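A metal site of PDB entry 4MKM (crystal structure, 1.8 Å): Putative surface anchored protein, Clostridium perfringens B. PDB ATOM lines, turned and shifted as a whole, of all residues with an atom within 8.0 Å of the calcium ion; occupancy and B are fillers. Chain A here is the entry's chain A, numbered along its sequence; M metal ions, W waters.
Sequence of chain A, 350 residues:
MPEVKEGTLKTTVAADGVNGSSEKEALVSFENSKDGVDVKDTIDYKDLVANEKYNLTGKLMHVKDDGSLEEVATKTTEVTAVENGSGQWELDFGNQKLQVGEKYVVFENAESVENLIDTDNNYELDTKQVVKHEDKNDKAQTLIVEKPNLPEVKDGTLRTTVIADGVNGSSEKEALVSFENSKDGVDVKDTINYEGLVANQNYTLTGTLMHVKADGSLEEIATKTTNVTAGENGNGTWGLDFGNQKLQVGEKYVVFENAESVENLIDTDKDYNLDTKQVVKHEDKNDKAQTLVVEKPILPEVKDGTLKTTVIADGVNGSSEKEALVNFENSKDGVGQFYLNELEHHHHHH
O of Gln 96 lies within hydrogen-bond range of N of Val 37, 2.7 Å away.
The backbone NH of Asp 16 lies within hydrogen-bond range of the backbone carbonyl oxygen of Asp 38, 2.9 Å away.
The side-chain hydroxyl of Ser 29 sits at hydrogen-bond distance from the side-chain amide nitrogen of Asn 32 (3.1 Å).
ND2 of Asn 95 sits at hydrogen-bond distance from O of Asp 35.
Residues that only touch the calcium ion: Val 37.
The calcium ion is bound by the backbone carbonyl oxygen of Gly 36 (2.1 Å), water W1 (2.2 Å), water W2 (2.2 Å), the side-chain carboxylate of Asp 35 (2.3 Å), the backbone carbonyl oxygen of Asn 32 (2.4 Å) and the side-chain carboxylate of Asp 16 (2.4 Å).
The calcium ion has six donor atoms within binding distance.
Slightly farther from the calcium ion lies the side-chain carboxylate (OD1) of Asp 16 (3.1 Å).
Water W2 lies within hydrogen-bond range of OD2 of Asp 38 (2.9 Å) and OD1 of Asp 16 (3.1 Å).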
ATOM      1  N   ALA A  15      -9.400  27.344  22.854  1.00  0.00           N
ATOM      2  CA  ALA A  15      -9.267  26.569  24.086  1.00  0.00           C
ATOM      3  C   ALA A  15      -7.799  26.605  24.457  1.00  0.00           C
ATOM      4  O   ALA A  15      -6.967  26.146  23.668  1.00  0.00           O
ATOM      5  CB  ALA A  15      -9.709  25.111  23.827  1.00  0.00           C
ATOM      6  N   ASP A  16      -7.466  27.226  25.598  1.00  0.00           N
ATOM      7  CA  ASP A  16      -6.087  27.463  26.049  1.00  0.00           C
ATOM      8  C   ASP A  16      -5.220  28.024  24.896  1.00  0.00           C
ATOM      9  O   ASP A  16      -4.092  27.587  24.678  1.00  0.00           O
ATOM     10  CB  ASP A  16      -5.473  26.202  26.719  1.00  0.00           C
ATOM     11  CG  ASP A  16      -5.826  25.976  28.197  1.00  0.00           C
ATOM     12  OD1 ASP A  16      -6.338  26.915  28.846  1.00  0.00           O
ATOM     13  OD2 ASP A  16      -5.545  24.865  28.712  1.00  0.00           O
ATOM     14  N   GLY A  17      -5.789  28.948  24.143  1.00  0.00           N
ATOM     15  CA  GLY A  17      -5.114  29.640  23.046  1.00  0.00           C
ATOM     16  C   GLY A  17      -5.039  28.946  21.704  1.00  0.00           C
ATOM     17  O   GLY A  17      -4.459  29.511  20.781  1.00  0.00           O
ATOM     18  N   VAL A  28      -6.370  20.407  23.013  1.00  0.00           N
ATOM     19  CA  VAL A  28      -5.808  20.900  24.273  1.00  0.00           C
ATOM     20  C   VAL A  28      -4.829  19.840  24.779  1.00  0.00           C
ATOM     21  O   VAL A  28      -5.227  18.711  25.005  1.00  0.00           O
ATOM     22  CB  VAL A  28      -6.888  21.240  25.317  1.00  0.00           C
ATOM     23  CG1 VAL A  28      -6.272  21.712  26.644  1.00  0.00           C
ATOM     24  CG2 VAL A  28      -7.881  22.268  24.775  1.00  0.00           C
ATOM     25  N   SER A  29      -3.538  20.170  24.921  1.00  0.00           N
ATOM     26  CA  SER A  29      -2.537  19.196  25.372  1.00  0.00           C
ATOM     27  C   SER A  29      -2.865  18.694  26.777  1.00  0.00           C
ATOM     28  O   SER A  29      -3.484  19.427  27.563  1.00  0.00           O
ATOM     29  CB  SER A  29      -1.136  19.827  25.403  1.00  0.00           C
ATOM     30  OG  SER A  29      -1.026  20.824  26.411  1.00  0.00           O
ATOM     31  N   PHE A  30      -2.454  17.467  27.095  1.00  0.00           N
ATOM     32  CA  PHE A  30      -2.645  16.896  28.439  1.00  0.00           C
ATOM     33  C   PHE A  30      -2.083  17.872  29.527  1.00  0.00           C
ATOM     34  O   PHE A  30      -2.774  18.142  30.510  1.00  0.00           O
ATOM     35  CB  PHE A  30      -1.959  15.518  28.562  1.00  0.00           C
ATOM     36  CG  PHE A  30      -2.054  14.975  29.968  1.00  0.00           C
ATOM     37  CD1 PHE A  30      -3.286  14.746  30.545  1.00  0.00           C
ATOM     38  CD2 PHE A  30      -0.922  14.868  30.760  1.00  0.00           C
ATOM     39  CE1 PHE A  30      -3.388  14.306  31.865  1.00  0.00           C
ATOM     40  CE2 PHE A  30      -1.022  14.409  32.068  1.00  0.00           C
ATOM     41  CZ  PHE A  30      -2.251  14.142  32.620  1.00  0.00           C
ATOM     42  N   GLU A  31      -0.885  18.429  29.300  1.00  0.00           N
ATOM     43  CA  GLU A  31      -0.236  19.373  30.244  1.00  0.00           C
ATOM     44  C   GLU A  31      -1.126  20.575  30.546  1.00  0.00           C
ATOM     45  O   GLU A  31      -1.333  20.908  31.717  1.00  0.00           O
ATOM     46  CB  GLU A  31       1.116  19.876  29.701  1.00  0.00           C
ATOM     47  N   ASN A  32      -1.684  21.195  29.489  1.00  0.00           N
ATOM     48  CA  ASN A  32      -2.542  22.355  29.635  1.00  0.00           C
ATOM     49  C   ASN A  32      -3.885  22.062  30.310  1.00  0.00           C
ATOM     50  O   ASN A  32      -4.395  22.934  30.989  1.00  0.00           O
ATOM     51  CB  ASN A  32      -2.697  23.100  28.314  1.00  0.00           C
ATOM     52  CG  ASN A  32      -1.394  23.718  27.842  1.00  0.00           C
ATOM     53  OD1 ASN A  32      -0.540  24.093  28.651  1.00  0.00           O
ATOM     54  ND2 ASN A  32      -1.231  23.900  26.544  1.00  0.00           N
ATOM     55  N   SER A  33      -4.397  20.829  30.214  1.00  0.00           N
ATOM     56  CA  SER A  33      -5.670  20.482  30.867  1.00  0.00           C
ATOM     57  C   SER A  33      -5.599  20.465  32.428  1.00  0.00           C
ATOM     58  O   SER A  33      -6.641  20.578  33.076  1.00  0.00           O
ATOM     59  CB  SER A  33      -6.139  19.098  30.389  1.00  0.00           C
ATOM     60  OG  SER A  33      -5.418  18.061  31.043  1.00  0.00           O
ATOM     61  N   LYS A  34      -4.393  20.315  33.008  1.00  0.00           N
ATOM     62  CA  LYS A  34      -4.168  20.148  34.461  1.00  0.00           C
ATOM     63  C   LYS A  34      -4.746  21.287  35.320  1.00  0.00           C
ATOM     64  O   LYS A  34      -5.289  21.007  36.394  1.00  0.00           O
ATOM     65  CB  LYS A  34      -2.676  19.936  34.750  1.00  0.00           C
ATOM     66  CG  LYS A  34      -2.105  18.628  34.179  1.00  0.00           C
ATOM     67  CD  LYS A  34      -0.553  18.628  34.246  1.00  0.00           C
ATOM     68  CE  LYS A  34       0.092  17.399  33.647  1.00  0.00           C
ATOM     69  NZ  LYS A  34       1.539  17.619  33.327  1.00  0.00           N
ATOM     70  N   ASP A  35      -4.665  22.533  34.853  1.00  0.00           N
ATOM     71  CA  ASP A  35      -5.188  23.690  35.591  1.00  0.00           C
ATOM     72  C   ASP A  35      -6.537  24.172  35.013  1.00  0.00           C
ATOM     73  O   ASP A  35      -6.909  25.321  35.232  1.00  0.00           O
ATOM     74  CB  ASP A  35      -4.143  24.850  35.587  1.00  0.00           C
ATOM     75  CG  ASP A  35      -3.799  25.454  34.225  1.00  0.00           C
ATOM     76  OD1 ASP A  35      -4.197  24.871  33.174  1.00  0.00           O
ATOM     77  OD2 ASP A  35      -3.051  26.454  34.199  1.00  0.00           O
ATOM     78  N   GLY A  36      -7.255  23.292  34.316  1.00  0.00           N
ATOM     79  CA  GLY A  36      -8.497  23.640  33.646  1.00  0.00           C
ATOM     80  C   GLY A  36      -8.187  24.156  32.249  1.00  0.00           C
ATOM     81  O   GLY A  36      -7.015  24.282  31.883  1.00  0.00           O
ATOM     82  N   VAL A  37      -9.230  24.447  31.444  1.00  0.00           N
ATOM     83  CA  VAL A  37      -9.086  24.984  30.078  1.00  0.00           C
ATOM     84  C   VAL A  37      -9.812  26.338  29.978  1.00  0.00           C
ATOM     85  O   VAL A  37     -10.956  26.440  30.384  1.00  0.00           O
ATOM     86  CB  VAL A  37      -9.648  23.988  29.022  1.00  0.00           C
ATOM     87  CG1 VAL A  37      -9.409  24.500  27.587  1.00  0.00           C
ATOM     88  CG2 VAL A  37      -9.069  22.590  29.216  1.00  0.00           C
ATOM     89  N   ASP A  38      -9.127  27.370  29.451  1.00  0.00           N
ATOM     90  CA  ASP A  38      -9.690  28.711  29.230  1.00  0.00           C
ATOM     91  C   ASP A  38     -10.406  28.636  27.900  1.00  0.00           C
ATOM     92  O   ASP A  38      -9.759  28.413  26.880  1.00  0.00           O
ATOM     93  CB  ASP A  38      -8.596  29.764  29.178  1.00  0.00           C
ATOM     94  CG  ASP A  38      -7.815  29.854  30.470  1.00  0.00           C
ATOM     95  OD1 ASP A  38      -8.434  30.124  31.521  1.00  0.00           O
ATOM     96  OD2 ASP A  38      -6.589  29.560  30.435  1.00  0.00           O
ATOM     97  N   ASN A  95     -12.182  29.832  32.856  1.00  0.00           N
ATOM     98  CA  ASN A  95     -11.602  28.525  33.150  1.00  0.00           C
ATOM     99  C   ASN A  95     -12.664  27.443  33.397  1.00  0.00           C
ATOM    100  O   ASN A  95     -13.548  27.621  34.257  1.00  0.00           O
ATOM    101  CB  ASN A  95     -10.710  28.634  34.357  1.00  0.00           C
ATOM    102  CG  ASN A  95      -9.910  27.389  34.623  1.00  0.00           C
ATOM    103  OD1 ASN A  95     -10.360  26.474  35.331  1.00  0.00           O
ATOM    104  ND2 ASN A  95      -8.688  27.344  34.083  1.00  0.00           N
ATOM    105  N   GLN A  96     -12.550  26.311  32.669  1.00  0.00           N
ATOM    106  CA  GLN A  96     -13.463  25.164  32.790  1.00  0.00           C
ATOM    107  C   GLN A  96     -12.684  23.914  33.110  1.00  0.00           C
ATOM    108  O   GLN A  96     -11.638  23.696  32.511  1.00  0.00           O
ATOM    109  CB  GLN A  96     -14.240  24.972  31.474  1.00  0.00           C
ATOM    110  CG  GLN A  96     -15.129  26.157  31.128  1.00  0.00           C
ATOM    111  CD  GLN A  96     -16.200  26.444  32.173  1.00  0.00           C
ATOM    112  OE1 GLN A  96     -16.776  25.520  32.757  1.00  0.00           O
ATOM    113  NE2 GLN A  96     -16.519  27.712  32.405  1.00  0.00           N
HETATM  114 CA    CA M   1      -5.252  25.181  31.114  1.00  0.00          CA
HETATM  115  O   HOH W   1      -3.348  25.790  30.294  1.00  0.00           O
HETATM  116  O   HOH W   2      -5.808  27.157  31.925  1.00  0.00           O
